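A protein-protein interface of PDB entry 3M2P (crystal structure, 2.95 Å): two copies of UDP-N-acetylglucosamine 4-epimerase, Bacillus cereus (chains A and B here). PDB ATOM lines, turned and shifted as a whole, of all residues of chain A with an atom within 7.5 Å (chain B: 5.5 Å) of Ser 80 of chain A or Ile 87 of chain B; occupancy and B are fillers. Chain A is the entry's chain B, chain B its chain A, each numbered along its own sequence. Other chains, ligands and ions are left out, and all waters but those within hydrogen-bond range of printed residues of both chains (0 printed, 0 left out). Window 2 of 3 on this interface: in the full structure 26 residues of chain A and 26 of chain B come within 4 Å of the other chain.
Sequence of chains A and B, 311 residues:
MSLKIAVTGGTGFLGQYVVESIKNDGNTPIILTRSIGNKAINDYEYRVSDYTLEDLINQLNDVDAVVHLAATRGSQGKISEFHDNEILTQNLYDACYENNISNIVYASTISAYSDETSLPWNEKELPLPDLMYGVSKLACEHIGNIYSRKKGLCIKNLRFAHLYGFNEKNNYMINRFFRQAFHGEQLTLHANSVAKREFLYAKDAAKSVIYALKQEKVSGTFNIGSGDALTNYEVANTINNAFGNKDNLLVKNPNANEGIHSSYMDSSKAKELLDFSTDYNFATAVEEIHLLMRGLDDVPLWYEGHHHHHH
NE2 of Gln 90 of chain B sits at hydrogen-bond distance from O of Gly 77 of chain A (2.9 Å). The backbone carbonyl oxygen (O) of His 83 of chain B sits at hydrogen-bond distance from a ring nitrogen (NE2) of His 83 of chain A (3.1 Å). The side-chain amide oxygen of Gln 90 of chain B sits at hydrogen-bond distance from the backbone NH of Ile 79 of chain A (2.9 Å).
The backbone NH (N) of Gly 77 of chain A sits at hydrogen-bond distance from the side-chain carboxylate (OE1) of Glu 81 of chain A, at 2.9 Å. O of Ile 87 of chain B sits close to OD1 of Asn 91 of chain B (3.5 Å). The side-chain carboxylate (OE1) of Glu 81 of chain A is in hydrogen-bond range of the backbone NH (N) of Lys 78 of chain A (2.9 Å). O of Ile 79 of chain A sits at hydrogen-bond distance from ND1 of His 83 of chain A (3.4 Å).
Among the printed residues, pairs that only touch across the chains: Lys 78 of chain A with Gln 90 of chain B, Ile 79 of chain A with Glu 86 of chain B, Ser 80 of chain A with Ile 87 of chain B, His 83 of chain A with Glu 86 of chain B, His 83 of chain A with Ile 87 of chain B and Met 132 of chain A with Gln 90 of chain B.
Of the printed residues of chain B, Gly 77 of chain A touches Gln 90. Printed residues of chain B within 4 Å of Lys 78 of chain A: Gln 90. Of the printed residues of chain B, Ile 79 of chain A touches Glu 86 and Gln 90. Of the printed residues of chain B, Ser 80 of chain A touches Ile 87. Glu 81 of chain A touches none of the printed residues of chain B. Phe 82 of chain A touches none of the printed residues of chain B. Of the printed residues of chain B, His 83 of chain A touches His 83 (3.1 Å), Glu 86 (3.2 Å) and Ile 87 (3.6 Å). Printed residues of chain B within 4 Å of Met 132 of chain A: Gln 90 (3.3 Å). Ile 87 of chain B touches just these residues of chain A: Ser 80 (3.6 Å) and His 83 (3.6 Å). The nearest residue of chain B that does not touch Ser 80 of chain A is Gln 90 of chain B (4.6 Å). The nearest residue of chain A that does not touch Ile 87 of chain B is Ile 79 of chain A (4.1 Å). The nearest printed residue of chain A that does not touch His 83 of chain B is Asp 84 of chain A (5.3 Å).
Printed residues of chain A that touch a printed residue of chain B: Gly 77, Lys 78, Ile 79, Ser 80, His 83 and Met 132. Hydrophobic or aromatic side chains of chain A that line the printed part of chain B: Ile 79, His 83 and Met 132.
His 83 of chain A touches its own counterpart, His 83 of chain B. 4 positions are printed for both chains. Of the 9 pairs that touch across the chains among the printed residues, 1 has its exchanged pair printed and touching as well.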
ATOM      1  N   GLN A  76       2.907  16.389  -1.078  1.00  0.00           N
ATOM      2  CA  GLN A  76       2.620  14.988  -1.381  1.00  0.00           C
ATOM      3  C   GLN A  76       2.715  14.569  -2.871  1.00  0.00           C
ATOM      4  O   GLN A  76       2.753  13.373  -3.181  1.00  0.00           O
ATOM      5  CB  GLN A  76       1.246  14.613  -0.813  1.00  0.00           C
ATOM      6  CG  GLN A  76       1.162  14.593   0.720  1.00  0.00           C
ATOM      7  CD  GLN A  76       1.939  13.434   1.322  1.00  0.00           C
ATOM      8  OE1 GLN A  76       3.168  13.487   1.438  1.00  0.00           O
ATOM      9  NE2 GLN A  76       1.223  12.378   1.709  1.00  0.00           N
ATOM     10  N   GLY A  77       2.757  15.533  -3.789  1.00  0.00           N
ATOM     11  CA  GLY A  77       2.655  15.205  -5.198  1.00  0.00           C
ATOM     12  C   GLY A  77       1.261  14.682  -5.515  1.00  0.00           C
ATOM     13  O   GLY A  77       1.084  13.773  -6.332  1.00  0.00           O
ATOM     14  N   LYS A  78       0.268  15.258  -4.844  1.00  0.00           N
ATOM     15  CA  LYS A  78      -1.140  14.938  -5.058  1.00  0.00           C
ATOM     16  C   LYS A  78      -1.869  16.165  -5.646  1.00  0.00           C
ATOM     17  O   LYS A  78      -1.722  17.285  -5.143  1.00  0.00           O
ATOM     18  CB  LYS A  78      -1.791  14.504  -3.736  1.00  0.00           C
ATOM     19  CG  LYS A  78      -1.094  13.352  -3.002  1.00  0.00           C
ATOM     20  CD  LYS A  78      -1.758  12.005  -3.269  1.00  0.00           C
ATOM     21  CE  LYS A  78      -1.365  11.426  -4.643  1.00  0.00           C
ATOM     22  NZ  LYS A  78      -0.146  10.528  -4.656  1.00  0.00           N
ATOM     23  N   ILE A  79      -2.640  15.955  -6.714  1.00  0.00           N
ATOM     24  CA  ILE A  79      -3.351  17.057  -7.358  1.00  0.00           C
ATOM     25  C   ILE A  79      -4.351  17.710  -6.397  1.00  0.00           C
ATOM     26  O   ILE A  79      -4.745  18.866  -6.573  1.00  0.00           O
ATOM     27  CB  ILE A  79      -4.090  16.613  -8.645  1.00  0.00           C
ATOM     28  CG1 ILE A  79      -4.361  17.819  -9.543  1.00  0.00           C
ATOM     29  CG2 ILE A  79      -5.394  15.907  -8.315  1.00  0.00           C
ATOM     30  CD1 ILE A  79      -3.112  18.430 -10.112  1.00  0.00           C
ATOM     31  N   SER A  80      -4.747  16.964  -5.374  1.00  0.00           N
ATOM     32  CA  SER A  80      -5.723  17.449  -4.421  1.00  0.00           C
ATOM     33  C   SER A  80      -5.164  18.573  -3.562  1.00  0.00           C
ATOM     34  O   SER A  80      -5.903  19.475  -3.173  1.00  0.00           O
ATOM     35  CB  SER A  80      -6.241  16.302  -3.549  1.00  0.00           C
ATOM     36  OG  SER A  80      -5.179  15.631  -2.890  1.00  0.00           O
ATOM     37  N   GLU A  81      -3.867  18.535  -3.271  1.00  0.00           N
ATOM     38  CA  GLU A  81      -3.263  19.546  -2.410  1.00  0.00           C
ATOM     39  C   GLU A  81      -3.405  20.930  -3.012  1.00  0.00           C
ATOM     40  O   GLU A  81      -3.272  21.937  -2.317  1.00  0.00           O
ATOM     41  CB  GLU A  81      -1.783  19.279  -2.197  1.00  0.00           C
ATOM     42  CG  GLU A  81      -1.416  17.930  -1.594  1.00  0.00           C
ATOM     43  CD  GLU A  81       0.095  17.699  -1.649  1.00  0.00           C
ATOM     44  OE1 GLU A  81       0.586  17.156  -2.663  1.00  0.00           O
ATOM     45  OE2 GLU A  81       0.800  18.103  -0.698  1.00  0.00           O
ATOM     46  N   PHE A  82      -3.677  20.978  -4.309  1.00  0.00           N
ATOM     47  CA  PHE A  82      -3.713  22.244  -5.030  1.00  0.00           C
ATOM     48  C   PHE A  82      -5.123  22.759  -5.361  1.00  0.00           C
ATOM     49  O   PHE A  82      -5.286  23.906  -5.771  1.00  0.00           O
ATOM     50  CB  PHE A  82      -2.872  22.131  -6.296  1.00  0.00           C
ATOM     51  CG  PHE A  82      -1.433  21.811  -6.034  1.00  0.00           C
ATOM     52  CD1 PHE A  82      -0.581  22.770  -5.521  1.00  0.00           C
ATOM     53  CD2 PHE A  82      -0.926  20.550  -6.302  1.00  0.00           C
ATOM     54  CE1 PHE A  82       0.740  22.485  -5.294  1.00  0.00           C
ATOM     55  CE2 PHE A  82       0.395  20.262  -6.073  1.00  0.00           C
ATOM     56  CZ  PHE A  82       1.224  21.229  -5.573  1.00  0.00           C
ATOM     57  N   HIS A  83      -6.129  21.913  -5.174  1.00  0.00           N
ATOM     58  CA  HIS A  83      -7.504  22.260  -5.497  1.00  0.00           C
ATOM     59  C   HIS A  83      -7.948  23.552  -4.821  1.00  0.00           C
ATOM     60  O   HIS A  83      -8.807  24.280  -5.313  1.00  0.00           O
ATOM     61  CB  HIS A  83      -8.442  21.142  -5.078  1.00  0.00           C
ATOM     62  CG  HIS A  83      -8.396  19.955  -5.972  1.00  0.00           C
ATOM     63  ND1 HIS A  83      -7.832  19.995  -7.230  1.00  0.00           N
ATOM     64  CD2 HIS A  83      -8.877  18.701  -5.811  1.00  0.00           C
ATOM     65  CE1 HIS A  83      -7.950  18.811  -7.797  1.00  0.00           C
ATOM     66  NE2 HIS A  83      -8.578  18.005  -6.958  1.00  0.00           N
ATOM     67  N   ASP A  84      -7.363  23.834  -3.674  1.00  0.00           N
ATOM     68  CA  ASP A  84      -7.734  25.014  -2.941  1.00  0.00           C
ATOM     69  C   ASP A  84      -7.294  26.266  -3.683  1.00  0.00           C
ATOM     70  O   ASP A  84      -8.065  27.199  -3.837  1.00  0.00           O
ATOM     71  CB  ASP A  84      -7.104  24.972  -1.559  1.00  0.00           C
ATOM     72  CG  ASP A  84      -8.021  25.508  -0.508  1.00  0.00           C
ATOM     73  OD1 ASP A  84      -9.054  24.841  -0.262  1.00  0.00           O
ATOM     74  OD2 ASP A  84      -7.717  26.592   0.053  1.00  0.00           O
ATOM     75  N   ASN A  85      -6.047  26.285  -4.132  1.00  0.00           N
ATOM     76  CA  ASN A  85      -5.536  27.399  -4.907  1.00  0.00           C
ATOM     77  C   ASN A  85      -6.458  27.724  -6.074  1.00  0.00           C
ATOM     78  O   ASN A  85      -6.587  28.878  -6.483  1.00  0.00           O
ATOM     79  CB  ASN A  85      -4.151  27.057  -5.438  1.00  0.00           C
ATOM     80  CG  ASN A  85      -3.106  27.041  -4.349  1.00  0.00           C
ATOM     81  OD1 ASN A  85      -2.194  26.201  -4.350  1.00  0.00           O
ATOM     82  ND2 ASN A  85      -3.229  27.975  -3.400  1.00  0.00           N
ATOM     83  N   MET A 132       2.436  18.004 -10.329  1.00  0.00           N
ATOM     84  CA  MET A 132       1.138  18.484  -9.872  1.00  0.00           C
ATOM     85  C   MET A 132       1.133  19.997  -9.640  1.00  0.00           C
ATOM     86  O   MET A 132       0.170  20.696  -9.958  1.00  0.00           O
ATOM     87  CB  MET A 132       0.783  17.780  -8.561  1.00  0.00           C
ATOM     88  CG  MET A 132      -0.191  16.635  -8.720  1.00  0.00           C
ATOM     89  SD  MET A 132      -0.134  15.807 -10.495  1.00  0.00           S
ATOM     90  CE  MET A 132      -1.696  14.668 -10.343  1.00  0.00           C
ATOM     91  N   TYR B  51     -13.730   4.529  -5.881  1.00  0.00           N
ATOM     92  CA  TYR B  51     -12.660   5.291  -6.524  1.00  0.00           C
ATOM     93  C   TYR B  51     -11.636   5.859  -5.547  1.00  0.00           C
ATOM     94  O   TYR B  51     -11.016   6.897  -5.788  1.00  0.00           O
ATOM     95  CB  TYR B  51     -13.222   6.360  -7.465  1.00  0.00           C
ATOM     96  CG  TYR B  51     -13.954   5.739  -8.629  1.00  0.00           C
ATOM     97  CD1 TYR B  51     -13.273   5.299  -9.758  1.00  0.00           C
ATOM     98  CD2 TYR B  51     -15.321   5.547  -8.577  1.00  0.00           C
ATOM     99  CE1 TYR B  51     -13.943   4.710 -10.799  1.00  0.00           C
ATOM    100  CE2 TYR B  51     -15.999   4.963  -9.616  1.00  0.00           C
ATOM    101  CZ  TYR B  51     -15.313   4.548 -10.723  1.00  0.00           C
ATOM    102  OH  TYR B  51     -16.026   3.980 -11.757  1.00  0.00           O
ATOM    103  N   PHE B  82     -15.229  19.630 -10.650  1.00  0.00           N
ATOM    104  CA  PHE B  82     -14.423  18.663 -11.373  1.00  0.00           C
ATOM    105  C   PHE B  82     -13.296  18.091 -10.529  1.00  0.00           C
ATOM    106  O   PHE B  82     -12.752  17.035 -10.832  1.00  0.00           O
ATOM    107  CB  PHE B  82     -13.855  19.316 -12.621  1.00  0.00           C
ATOM    108  CG  PHE B  82     -14.903  19.772 -13.579  1.00  0.00           C
ATOM    109  CD1 PHE B  82     -15.585  18.860 -14.352  1.00  0.00           C
ATOM    110  CD2 PHE B  82     -15.212  21.115 -13.700  1.00  0.00           C
ATOM    111  CE1 PHE B  82     -16.549  19.275 -15.231  1.00  0.00           C
ATOM    112  CE2 PHE B  82     -16.180  21.537 -14.578  1.00  0.00           C
ATOM    113  CZ  PHE B  82     -16.849  20.616 -15.345  1.00  0.00           C
ATOM    114  N   HIS B  83     -12.955  18.791  -9.459  1.00  0.00           N
ATOM    115  CA  HIS B  83     -11.863  18.391  -8.600  1.00  0.00           C
ATOM    116  C   HIS B  83     -11.976  16.943  -8.152  1.00  0.00           C
ATOM    117  O   HIS B  83     -10.980  16.284  -7.886  1.00  0.00           O
ATOM    118  CB  HIS B  83     -11.781  19.327  -7.403  1.00  0.00           C
ATOM    119  CG  HIS B  83     -11.186  20.652  -7.729  1.00  0.00           C
ATOM    120  ND1 HIS B  83     -10.384  20.851  -8.831  1.00  0.00           N
ATOM    121  CD2 HIS B  83     -11.246  21.844  -7.094  1.00  0.00           C
ATOM    122  CE1 HIS B  83      -9.995  22.111  -8.873  1.00  0.00           C
ATOM    123  NE2 HIS B  83     -10.501  22.735  -7.825  1.00  0.00           N
ATOM    124  N   ASP B  84     -13.189  16.434  -8.068  1.00  0.00           N
ATOM    125  CA  ASP B  84     -13.363  15.055  -7.653  1.00  0.00           C
ATOM    126  C   ASP B  84     -12.879  14.100  -8.739  1.00  0.00           C
ATOM    127  O   ASP B  84     -12.326  13.050  -8.445  1.00  0.00           O
ATOM    128  CB  ASP B  84     -14.817  14.781  -7.304  1.00  0.00           C
ATOM    129  CG  ASP B  84     -14.968  13.618  -6.368  1.00  0.00           C
ATOM    130  OD1 ASP B  84     -15.077  13.857  -5.143  1.00  0.00           O
ATOM    131  OD2 ASP B  84     -14.956  12.464  -6.854  1.00  0.00           O
ATOM    132  N   ASN B  85     -13.096  14.474  -9.995  1.00  0.00           N
ATOM    133  CA  ASN B  85     -12.531  13.771 -11.135  1.00  0.00           C
ATOM    134  C   ASN B  85     -11.017  13.743 -11.113  1.00  0.00           C
ATOM    135  O   ASN B  85     -10.404  12.681 -11.154  1.00  0.00           O
ATOM    136  CB  ASN B  85     -12.961  14.451 -12.423  1.00  0.00           C
ATOM    137  CG  ASN B  85     -14.186  13.835 -13.006  1.00  0.00           C
ATOM    138  OD1 ASN B  85     -15.220  14.492 -13.139  1.00  0.00           O
ATOM    139  ND2 ASN B  85     -14.094  12.554 -13.355  1.00  0.00           N
ATOM    140  N   GLU B  86     -10.413  14.923 -11.082  1.00  0.00           N
ATOM    141  CA  GLU B  86      -8.968  15.016 -11.029  1.00  0.00           C
ATOM    142  C   GLU B  86      -8.415  14.015 -10.008  1.00  0.00           C
ATOM    143  O   GLU B  86      -7.540  13.211 -10.319  1.00  0.00           O
ATOM    144  CB  GLU B  86      -8.537  16.462 -10.759  1.00  0.00           C
ATOM    145  CG  GLU B  86      -8.982  17.396 -11.880  1.00  0.00           C
ATOM    146  CD  GLU B  86      -8.434  18.807 -11.768  1.00  0.00           C
ATOM    147  OE1 GLU B  86      -7.516  19.034 -10.953  1.00  0.00           O
ATOM    148  OE2 GLU B  86      -8.927  19.695 -12.507  1.00  0.00           O
ATOM    149  N   ILE B  87      -8.972  14.037  -8.807  1.00  0.00           N
ATOM    150  CA  ILE B  87      -8.630  13.073  -7.767  1.00  0.00           C
ATOM    151  C   ILE B  87      -8.879  11.626  -8.210  1.00  0.00           C
ATOM    152  O   ILE B  87      -8.027  10.771  -8.046  1.00  0.00           O
ATOM    153  CB  ILE B  87      -9.411  13.394  -6.456  1.00  0.00           C
ATOM    154  CG1 ILE B  87      -8.838  14.653  -5.805  1.00  0.00           C
ATOM    155  CG2 ILE B  87      -9.415  12.217  -5.495  1.00  0.00           C
ATOM    156  CD1 ILE B  87      -9.402  14.933  -4.488  1.00  0.00           C
ATOM    157  N   LEU B  88     -10.051  11.356  -8.762  1.00  0.00           N
ATOM    158  CA  LEU B  88     -10.401  10.011  -9.178  1.00  0.00           C
ATOM    159  C   LEU B  88      -9.357   9.515 -10.172  1.00  0.00           C
ATOM    160  O   LEU B  88      -8.967   8.353 -10.160  1.00  0.00           O
ATOM    161  CB  LEU B  88     -11.805  10.007  -9.809  1.00  0.00           C
ATOM    162  CG  LEU B  88     -12.434   8.659 -10.189  1.00  0.00           C
ATOM    163  CD1 LEU B  88     -13.902   8.799 -10.474  1.00  0.00           C
ATOM    164  CD2 LEU B  88     -11.737   8.017 -11.379  1.00  0.00           C
ATOM    165  N   THR B  89      -8.909  10.421 -11.033  1.00  0.00           N
ATOM    166  CA  THR B  89      -7.940  10.103 -12.063  1.00  0.00           C
ATOM    167  C   THR B  89      -6.606   9.684 -11.456  1.00  0.00           C
ATOM    168  O   THR B  89      -6.166   8.561 -11.670  1.00  0.00           O
ATOM    169  CB  THR B  89      -7.790  11.280 -13.056  1.00  0.00           C
ATOM    170  OG1 THR B  89      -8.900  11.265 -13.958  1.00  0.00           O
ATOM    171  CG2 THR B  89      -6.507  11.183 -13.866  1.00  0.00           C
ATOM    172  N   GLN B  90      -5.981  10.568 -10.679  1.00  0.00           N
ATOM    173  CA  GLN B  90      -4.738  10.232  -9.977  1.00  0.00           C
ATOM    174  C   GLN B  90      -4.820   8.960  -9.143  1.00  0.00           C
ATOM    175  O   GLN B  90      -3.847   8.220  -9.057  1.00  0.00           O
ATOM    176  CB  GLN B  90      -4.240  11.375  -9.096  1.00  0.00           C
ATOM    177  CG  GLN B  90      -2.868  11.091  -8.503  1.00  0.00           C
ATOM    178  CD  GLN B  90      -2.227  12.316  -7.884  1.00  0.00           C
ATOM    179  OE1 GLN B  90      -2.905  13.157  -7.303  1.00  0.00           O
ATOM    180  NE2 GLN B  90      -0.911  12.420  -8.001  1.00  0.00           N
ATOM    181  N   ASN B  91      -5.967   8.706  -8.528  1.00  0.00           N
ATOM    182  CA  ASN B  91      -6.144   7.476  -7.768  1.00  0.00           C
ATOM    183  C   ASN B  91      -5.965   6.291  -8.682  1.00  0.00           C
ATOM    184  O   ASN B  91      -5.209   5.359  -8.394  1.00  0.00           O
ATOM    185  CB  ASN B  91      -7.542   7.393  -7.160  1.00  0.00           C
ATOM    186  CG  ASN B  91      -7.701   8.248  -5.926  1.00  0.00           C
ATOM    187  OD1 ASN B  91      -8.820   8.521  -5.506  1.00  0.00           O
ATOM    188  ND2 ASN B  91      -6.588   8.682  -5.345  1.00  0.00           N
ATOM    189  N   LEU B  92      -6.699   6.338  -9.787  1.00  0.00           N
ATOM    190  CA  LEU B  92      -6.692   5.283 -10.789  1.00  0.00           C
ATOM    191  C   LEU B  92      -5.282   4.986 -11.290  1.00  0.00           C
ATOM    192  O   LEU B  92      -4.883   3.829 -11.363  1.00  0.00           O
ATOM    193  CB  LEU B  92      -7.595   5.679 -11.953  1.00  0.00           C
ATOM    194  CG  LEU B  92      -7.891   4.591 -12.966  1.00  0.00           C
ATOM    195  CD1 LEU B  92      -8.792   3.535 -12.346  1.00  0.00           C
ATOM    196  CD2 LEU B  92      -8.517   5.228 -14.186  1.00  0.00           C
